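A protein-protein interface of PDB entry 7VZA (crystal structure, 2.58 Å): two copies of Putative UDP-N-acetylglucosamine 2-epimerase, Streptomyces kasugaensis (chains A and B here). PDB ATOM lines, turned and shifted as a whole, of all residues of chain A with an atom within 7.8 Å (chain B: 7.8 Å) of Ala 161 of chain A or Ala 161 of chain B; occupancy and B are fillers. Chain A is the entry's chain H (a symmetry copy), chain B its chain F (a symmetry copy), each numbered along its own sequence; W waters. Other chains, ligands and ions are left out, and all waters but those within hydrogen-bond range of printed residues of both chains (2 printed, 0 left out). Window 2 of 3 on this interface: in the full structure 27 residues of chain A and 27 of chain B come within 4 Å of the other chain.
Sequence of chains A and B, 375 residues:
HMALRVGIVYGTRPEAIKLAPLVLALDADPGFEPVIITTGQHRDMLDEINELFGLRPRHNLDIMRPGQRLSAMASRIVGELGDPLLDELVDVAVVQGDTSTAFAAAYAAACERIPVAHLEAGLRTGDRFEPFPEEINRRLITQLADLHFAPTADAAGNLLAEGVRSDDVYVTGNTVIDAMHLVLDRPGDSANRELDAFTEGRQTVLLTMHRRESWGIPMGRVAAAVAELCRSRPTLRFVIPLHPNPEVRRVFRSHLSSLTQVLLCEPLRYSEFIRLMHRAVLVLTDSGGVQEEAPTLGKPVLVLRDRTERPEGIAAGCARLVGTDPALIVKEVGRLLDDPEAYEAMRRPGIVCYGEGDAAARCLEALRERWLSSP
The backbone carbonyl oxygen of Ala 161 of chain B is in hydrogen-bond range of the backbone NH of Gly 163 of chain A. The backbone NH (N) of Gly 163 of chain B sits at hydrogen-bond distance from the backbone carbonyl oxygen (O) of Ala 161 of chain A, at 3.4 Å. The backbone carbonyl oxygen (O) of Ala 161 of chain B sits close to the backbone carbonyl oxygen (O) of Ala 161 of chain A (3.5 Å).
NE of Arg 124 of chain B lies within salt-bridge range of OE2 of Glu 162 of chain B, at 2.7 Å. The side-chain amide nitrogen (NE2) of Gln 143 of chain B sits at hydrogen-bond distance from the backbone carbonyl oxygen (O) of Glu 162 of chain B, at 3.1 Å. NE of Arg 124 of chain A is in salt-bridge range of OE2 of Glu 162 of chain A (2.7 Å). The backbone carbonyl oxygen (O) of Glu 162 of chain A sits at hydrogen-bond distance from the side-chain amide nitrogen (NE2) of Gln 143 of chain A, at 3.2 Å.
Among the printed residues, merely in contact across the chains: Glu 162 of chain A with Glu 162 of chain B (3.5 Å), Glu 162 of chain A with Ala 161 of chain B (3.7 Å), Ala 161 of chain A with Glu 162 of chain B (3.8 Å) and Gln 143 of chain A with Gln 143 of chain B (3.9 Å).
Printed residues of chain A within 4 Å of Ala 161 of chain B: Ala 161, Glu 162 and Gly 163. Of the printed residues of chain A, Glu 162 of chain B touches Ala 161 and Glu 162. Of the printed residues of chain A, Gly 163 of chain B touches Ala 161. The nearest residue of chain B that does not touch Ala 161 of chain A is Leu 160 of chain B (4.5 Å). The nearest printed residue of chain A that does not touch Glu 162 of chain B is Gly 163 of chain A (4.2 Å).
Of the 13 printed residues of chain B, 4 touch a printed residue of chain A. Printed residues of chain B that touch a printed residue of chain A: Gln 143, Ala 161, Glu 162 and Gly 163.
Gln 143 of chain A touches its own counterpart, Gln 143 of chain B. Ala 161 of chain B touches its own counterpart, Ala 161 of chain A. Ala 161 of chain A touches Gly 163 of chain B, and with the chains exchanged Gly 163 of chain A touches Ala 161 of chain B. Glu 162 of chain B touches its own counterpart, Glu 162 of chain A. Positions printed for both chains: 124, 142, 143, 155, 156, 157, 158, 159, 160, 161, 162, 163 and 164. Of the 7 pairs that touch across the chains among the printed residues, 7 have their exchanged pair printed and touching as well.
Water W2 bridges O of Ala 161 of chain B (2.5 Å) and O of Leu 160 of chain A (3.2 Å). Water W1 lies within hydrogen-bond range of the side-chain carboxylate (OE1) of Glu 162 of chain B, the side-chain amide nitrogen (NE2) of Gln 143 of chain B and the side-chain amide oxygen (OE1) of Gln 143 of chain A.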
ATOM      1  N   ARG A 124     -14.732 -25.022 -14.628  1.00  0.00           N
ATOM      2  CA  ARG A 124     -13.303 -25.343 -14.914  1.00  0.00           C
ATOM      3  C   ARG A 124     -12.528 -25.381 -13.591  1.00  0.00           C
ATOM      4  O   ARG A 124     -12.788 -24.535 -12.741  1.00  0.00           O
ATOM      5  CB  ARG A 124     -12.686 -24.312 -15.863  1.00  0.00           C
ATOM      6  CG  ARG A 124     -13.344 -24.214 -17.229  1.00  0.00           C
ATOM      7  CD  ARG A 124     -13.021 -25.399 -18.127  1.00  0.00           C
ATOM      8  NE  ARG A 124     -13.621 -25.317 -19.458  1.00  0.00           N
ATOM      9  CZ  ARG A 124     -14.891 -25.615 -19.759  1.00  0.00           C
ATOM     10  NH1 ARG A 124     -15.724 -26.042 -18.825  1.00  0.00           N
ATOM     11  NH2 ARG A 124     -15.309 -25.541 -21.014  1.00  0.00           N
ATOM     12  N   THR A 142     -18.206 -28.692 -24.992  1.00  0.00           N
ATOM     13  CA  THR A 142     -18.255 -27.219 -25.181  1.00  0.00           C
ATOM     14  C   THR A 142     -18.170 -26.894 -26.676  1.00  0.00           C
ATOM     15  O   THR A 142     -18.916 -25.992 -27.109  1.00  0.00           O
ATOM     16  CB  THR A 142     -17.180 -26.516 -24.340  1.00  0.00           C
ATOM     17  OG1 THR A 142     -17.641 -26.524 -22.988  1.00  0.00           O
ATOM     18  CG2 THR A 142     -16.915 -25.099 -24.782  1.00  0.00           C
ATOM     19  N   GLN A 143     -17.324 -27.603 -27.433  1.00  0.00           N
ATOM     20  CA  GLN A 143     -17.154 -27.375 -28.890  1.00  0.00           C
ATOM     21  C   GLN A 143     -18.322 -27.997 -29.668  1.00  0.00           C
ATOM     22  O   GLN A 143     -18.618 -27.492 -30.752  1.00  0.00           O
ATOM     23  CB  GLN A 143     -15.813 -27.913 -29.394  1.00  0.00           C
ATOM     24  CG  GLN A 143     -14.601 -27.239 -28.760  1.00  0.00           C
ATOM     25  CD  GLN A 143     -14.567 -25.733 -28.913  1.00  0.00           C
ATOM     26  OE1 GLN A 143     -14.802 -25.184 -29.984  1.00  0.00           O
ATOM     27  NE2 GLN A 143     -14.236 -25.055 -27.835  1.00  0.00           N
ATOM     28  N   ALA A 155     -18.711 -19.113 -14.972  1.00  0.00           N
ATOM     29  CA  ALA A 155     -18.808 -20.244 -15.925  1.00  0.00           C
ATOM     30  C   ALA A 155     -18.989 -19.710 -17.352  1.00  0.00           C
ATOM     31  O   ALA A 155     -18.320 -20.223 -18.275  1.00  0.00           O
ATOM     32  CB  ALA A 155     -19.934 -21.170 -15.525  1.00  0.00           C
ATOM     33  N   ALA A 156     -19.844 -18.706 -17.532  1.00  0.00           N
ATOM     34  CA  ALA A 156     -20.073 -18.068 -18.845  1.00  0.00           C
ATOM     35  C   ALA A 156     -18.746 -17.517 -19.379  1.00  0.00           C
ATOM     36  O   ALA A 156     -18.461 -17.704 -20.573  1.00  0.00           O
ATOM     37  CB  ALA A 156     -21.135 -17.006 -18.723  1.00  0.00           C
ATOM     38  N   GLY A 157     -17.949 -16.890 -18.516  1.00  0.00           N
ATOM     39  CA  GLY A 157     -16.633 -16.345 -18.894  1.00  0.00           C
ATOM     40  C   GLY A 157     -15.710 -17.429 -19.433  1.00  0.00           C
ATOM     41  O   GLY A 157     -15.042 -17.199 -20.461  1.00  0.00           O
ATOM     42  N   ASN A 158     -15.683 -18.580 -18.762  1.00  0.00           N
ATOM     43  CA  ASN A 158     -14.819 -19.726 -19.140  1.00  0.00           C
ATOM     44  C   ASN A 158     -15.179 -20.193 -20.560  1.00  0.00           C
ATOM     45  O   ASN A 158     -14.251 -20.533 -21.324  1.00  0.00           O
ATOM     46  CB  ASN A 158     -14.931 -20.850 -18.114  1.00  0.00           C
ATOM     47  CG  ASN A 158     -14.359 -20.477 -16.760  1.00  0.00           C
ATOM     48  OD1 ASN A 158     -13.516 -19.596 -16.647  1.00  0.00           O
ATOM     49  ND2 ASN A 158     -14.800 -21.152 -15.716  1.00  0.00           N
ATOM     50  N   LEU A 159     -16.465 -20.184 -20.919  1.00  0.00           N
ATOM     51  CA  LEU A 159     -16.922 -20.568 -22.280  1.00  0.00           C
ATOM     52  C   LEU A 159     -16.398 -19.560 -23.310  1.00  0.00           C
ATOM     53  O   LEU A 159     -15.853 -20.007 -24.341  1.00  0.00           O
ATOM     54  CB  LEU A 159     -18.451 -20.666 -22.294  1.00  0.00           C
ATOM     55  CG  LEU A 159     -19.023 -21.742 -21.375  1.00  0.00           C
ATOM     56  CD1 LEU A 159     -20.517 -21.594 -21.191  1.00  0.00           C
ATOM     57  CD2 LEU A 159     -18.687 -23.142 -21.894  1.00  0.00           C
ATOM     58  N   LEU A 160     -16.500 -18.258 -23.026  1.00  0.00           N
ATOM     59  CA  LEU A 160     -16.013 -17.183 -23.944  1.00  0.00           C
ATOM     60  C   LEU A 160     -14.513 -17.379 -24.199  1.00  0.00           C
ATOM     61  O   LEU A 160     -14.080 -17.190 -25.342  1.00  0.00           O
ATOM     62  CB  LEU A 160     -16.294 -15.795 -23.352  1.00  0.00           C
ATOM     63  CG  LEU A 160     -17.767 -15.446 -23.101  1.00  0.00           C
ATOM     64  CD1 LEU A 160     -17.933 -13.972 -22.781  1.00  0.00           C
ATOM     65  CD2 LEU A 160     -18.643 -15.843 -24.272  1.00  0.00           C
ATOM     66  N   ALA A 161     -13.763 -17.797 -23.179  1.00  0.00           N
ATOM     67  CA  ALA A 161     -12.296 -17.996 -23.237  1.00  0.00           C
ATOM     68  C   ALA A 161     -11.940 -19.189 -24.144  1.00  0.00           C
ATOM     69  O   ALA A 161     -10.767 -19.274 -24.571  1.00  0.00           O
ATOM     70  CB  ALA A 161     -11.756 -18.174 -21.838  1.00  0.00           C
ATOM     71  N   GLU A 162     -12.897 -20.088 -24.414  1.00  0.00           N
ATOM     72  CA  GLU A 162     -12.683 -21.272 -25.290  1.00  0.00           C
ATOM     73  C   GLU A 162     -13.345 -21.036 -26.652  1.00  0.00           C
ATOM     74  O   GLU A 162     -13.439 -22.012 -27.451  1.00  0.00           O
ATOM     75  CB  GLU A 162     -13.179 -22.540 -24.589  1.00  0.00           C
ATOM     76  CG  GLU A 162     -12.208 -23.040 -23.534  1.00  0.00           C
ATOM     77  CD  GLU A 162     -12.766 -24.073 -22.579  1.00  0.00           C
ATOM     78  OE1 GLU A 162     -13.673 -24.837 -22.999  1.00  0.00           O
ATOM     79  OE2 GLU A 162     -12.287 -24.124 -21.425  1.00  0.00           O
ATOM     80  N   GLY A 163     -13.769 -19.797 -26.923  1.00  0.00           N
ATOM     81  CA  GLY A 163     -14.095 -19.330 -28.286  1.00  0.00           C
ATOM     82  C   GLY A 163     -15.579 -19.401 -28.586  1.00  0.00           C
ATOM     83  O   GLY A 163     -15.963 -19.191 -29.731  1.00  0.00           O
ATOM     84  N   VAL A 164     -16.400 -19.689 -27.583  1.00  0.00           N
ATOM     85  CA  VAL A 164     -17.880 -19.760 -27.750  1.00  0.00           C
ATOM     86  C   VAL A 164     -18.394 -18.325 -27.947  1.00  0.00           C
ATOM     87  O   VAL A 164     -17.961 -17.424 -27.205  1.00  0.00           O
ATOM     88  CB  VAL A 164     -18.522 -20.458 -26.544  1.00  0.00           C
ATOM     89  CG1 VAL A 164     -20.033 -20.469 -26.629  1.00  0.00           C
ATOM     90  CG2 VAL A 164     -18.000 -21.872 -26.392  1.00  0.00           C
ATOM     91  N   ARG B 124      -9.179 -22.162 -39.616  1.00  0.00           N
ATOM     92  CA  ARG B 124     -10.612 -21.885 -39.324  1.00  0.00           C
ATOM     93  C   ARG B 124     -11.202 -21.136 -40.523  1.00  0.00           C
ATOM     94  O   ARG B 124     -10.514 -20.256 -41.067  1.00  0.00           O
ATOM     95  CB  ARG B 124     -10.782 -21.055 -38.047  1.00  0.00           C
ATOM     96  CG  ARG B 124     -10.246 -21.702 -36.778  1.00  0.00           C
ATOM     97  CD  ARG B 124     -11.108 -22.836 -36.275  1.00  0.00           C
ATOM     98  NE  ARG B 124     -10.633 -23.447 -35.030  1.00  0.00           N
ATOM     99  CZ  ARG B 124      -9.663 -24.361 -34.946  1.00  0.00           C
ATOM    100  NH1 ARG B 124      -9.029 -24.787 -36.027  1.00  0.00           N
ATOM    101  NH2 ARG B 124      -9.344 -24.875 -33.769  1.00  0.00           N
ATOM    102  N   THR B 142      -8.410 -30.024 -31.203  1.00  0.00           N
ATOM    103  CA  THR B 142      -7.718 -28.863 -30.578  1.00  0.00           C
ATOM    104  C   THR B 142      -7.741 -29.015 -29.055  1.00  0.00           C
ATOM    105  O   THR B 142      -6.700 -28.728 -28.440  1.00  0.00           O
ATOM    106  CB  THR B 142      -8.307 -27.538 -31.074  1.00  0.00           C
ATOM    107  OG1 THR B 142      -7.811 -27.343 -32.401  1.00  0.00           O
ATOM    108  CG2 THR B 142      -7.948 -26.367 -30.194  1.00  0.00           C
ATOM    109  N   GLN B 143      -8.854 -29.476 -28.479  1.00  0.00           N
ATOM    110  CA  GLN B 143      -8.989 -29.673 -27.007  1.00  0.00           C
ATOM    111  C   GLN B 143      -8.270 -30.957 -26.570  1.00  0.00           C
ATOM    112  O   GLN B 143      -7.831 -30.998 -25.418  1.00  0.00           O
ATOM    113  CB  GLN B 143     -10.459 -29.700 -26.575  1.00  0.00           C
ATOM    114  CG  GLN B 143     -11.217 -28.415 -26.868  1.00  0.00           C
ATOM    115  CD  GLN B 143     -10.595 -27.179 -26.255  1.00  0.00           C
ATOM    116  OE1 GLN B 143     -10.206 -27.156 -25.092  1.00  0.00           O
ATOM    117  NE2 GLN B 143     -10.523 -26.121 -27.044  1.00  0.00           N
ATOM    118  N   ALA B 155      -3.035 -19.061 -37.755  1.00  0.00           N
ATOM    119  CA  ALA B 155      -3.510 -20.358 -37.219  1.00  0.00           C
ATOM    120  C   ALA B 155      -3.215 -20.444 -35.717  1.00  0.00           C
ATOM    121  O   ALA B 155      -4.107 -20.872 -34.946  1.00  0.00           O
ATOM    122  CB  ALA B 155      -2.884 -21.500 -37.979  1.00  0.00           C
ATOM    123  N   ALA B 156      -2.021 -20.033 -35.297  1.00  0.00           N
ATOM    124  CA  ALA B 156      -1.627 -20.020 -33.873  1.00  0.00           C
ATOM    125  C   ALA B 156      -2.606 -19.142 -33.086  1.00  0.00           C
ATOM    126  O   ALA B 156      -3.027 -19.551 -31.998  1.00  0.00           O
ATOM    127  CB  ALA B 156      -0.200 -19.552 -33.740  1.00  0.00           C
ATOM    128  N   GLY B 157      -2.985 -17.989 -33.638  1.00  0.00           N
ATOM    129  CA  GLY B 157      -3.946 -17.070 -33.001  1.00  0.00           C
ATOM    130  C   GLY B 157      -5.283 -17.737 -32.761  1.00  0.00           C
ATOM    131  O   GLY B 157      -5.850 -17.566 -31.653  1.00  0.00           O
ATOM    132  N   ASN B 158      -5.771 -18.487 -33.756  1.00  0.00           N
ATOM    133  CA  ASN B 158      -7.075 -19.195 -33.678  1.00  0.00           C
ATOM    134  C   ASN B 158      -7.062 -20.179 -32.506  1.00  0.00           C
ATOM    135  O   ASN B 158      -8.090 -20.280 -31.809  1.00  0.00           O
ATOM    136  CB  ASN B 158      -7.403 -19.864 -35.007  1.00  0.00           C
ATOM    137  CG  ASN B 158      -7.663 -18.870 -36.120  1.00  0.00           C
ATOM    138  OD1 ASN B 158      -8.046 -17.731 -35.869  1.00  0.00           O
ATOM    139  ND2 ASN B 158      -7.484 -19.295 -37.361  1.00  0.00           N
ATOM    140  N   LEU B 159      -5.934 -20.856 -32.272  1.00  0.00           N
ATOM    141  CA  LEU B 159      -5.793 -21.818 -31.144  1.00  0.00           C
ATOM    142  C   LEU B 159      -5.876 -21.058 -29.815  1.00  0.00           C
ATOM    143  O   LEU B 159      -6.629 -21.517 -28.929  1.00  0.00           O
ATOM    144  CB  LEU B 159      -4.475 -22.581 -31.286  1.00  0.00           C
ATOM    145  CG  LEU B 159      -4.362 -23.434 -32.546  1.00  0.00           C
ATOM    146  CD1 LEU B 159      -2.928 -23.886 -32.782  1.00  0.00           C
ATOM    147  CD2 LEU B 159      -5.298 -24.625 -32.473  1.00  0.00           C
ATOM    148  N   LEU B 160      -5.182 -19.921 -29.683  1.00  0.00           N
ATOM    149  CA  LEU B 160      -5.194 -19.094 -28.438  1.00  0.00           C
ATOM    150  C   LEU B 160      -6.632 -18.677 -28.125  1.00  0.00           C
ATOM    151  O   LEU B 160      -7.002 -18.691 -26.946  1.00  0.00           O
ATOM    152  CB  LEU B 160      -4.286 -17.868 -28.592  1.00  0.00           C
ATOM    153  CG  LEU B 160      -2.798 -18.150 -28.852  1.00  0.00           C
ATOM    154  CD1 LEU B 160      -1.960 -16.893 -28.705  1.00  0.00           C
ATOM    155  CD2 LEU B 160      -2.263 -19.259 -27.959  1.00  0.00           C
ATOM    156  N   ALA B 161      -7.425 -18.367 -29.155  1.00  0.00           N
ATOM    157  CA  ALA B 161      -8.827 -17.901 -29.027  1.00  0.00           C
ATOM    158  C   ALA B 161      -9.733 -19.029 -28.512  1.00  0.00           C
ATOM    159  O   ALA B 161     -10.840 -18.714 -28.017  1.00  0.00           O
ATOM    160  CB  ALA B 161      -9.303 -17.371 -30.357  1.00  0.00           C
ATOM    161  N   GLU B 162      -9.303 -20.292 -28.627  1.00  0.00           N
ATOM    162  CA  GLU B 162     -10.082 -21.467 -28.150  1.00  0.00           C
ATOM    163  C   GLU B 162      -9.465 -22.004 -26.852  1.00  0.00           C
ATOM    164  O   GLU B 162      -9.868 -23.107 -26.414  1.00  0.00           O
ATOM    165  CB  GLU B 162     -10.165 -22.516 -29.259  1.00  0.00           C
ATOM    166  CG  GLU B 162     -11.178 -22.174 -30.333  1.00  0.00           C
ATOM    167  CD  GLU B 162     -11.054 -22.993 -31.613  1.00  0.00           C
ATOM    168  OE1 GLU B 162     -10.606 -24.159 -31.530  1.00  0.00           O
ATOM    169  OE2 GLU B 162     -11.425 -22.461 -32.695  1.00  0.00           O
ATOM    170  N   GLY B 163      -8.553 -21.239 -26.239  1.00  0.00           N
ATOM    171  CA  GLY B 163      -8.143 -21.425 -24.836  1.00  0.00           C
ATOM    172  C   GLY B 163      -6.857 -22.218 -24.708  1.00  0.00           C
ATOM    173  O   GLY B 163      -6.474 -22.519 -23.568  1.00  0.00           O
ATOM    174  N   VAL B 164      -6.191 -22.520 -25.815  1.00  0.00           N
ATOM    175  CA  VAL B 164      -4.905 -23.261 -25.807  1.00  0.00           C
ATOM    176  C   VAL B 164      -3.820 -22.351 -25.222  1.00  0.00           C
ATOM    177  O   VAL B 164      -3.759 -21.174 -25.609  1.00  0.00           O
ATOM    178  CB  VAL B 164      -4.554 -23.747 -27.226  1.00  0.00           C
ATOM    179  CG1 VAL B 164      -3.204 -24.440 -27.293  1.00  0.00           C
ATOM    180  CG2 VAL B 164      -5.635 -24.670 -27.764  1.00  0.00           C
HETATM  181  O   HOH W   1     -11.486 -25.940 -29.741  1.00  0.00           O
HETATM  182  O   HOH W   2     -12.326 -16.656 -28.001  1.00  0.00           O
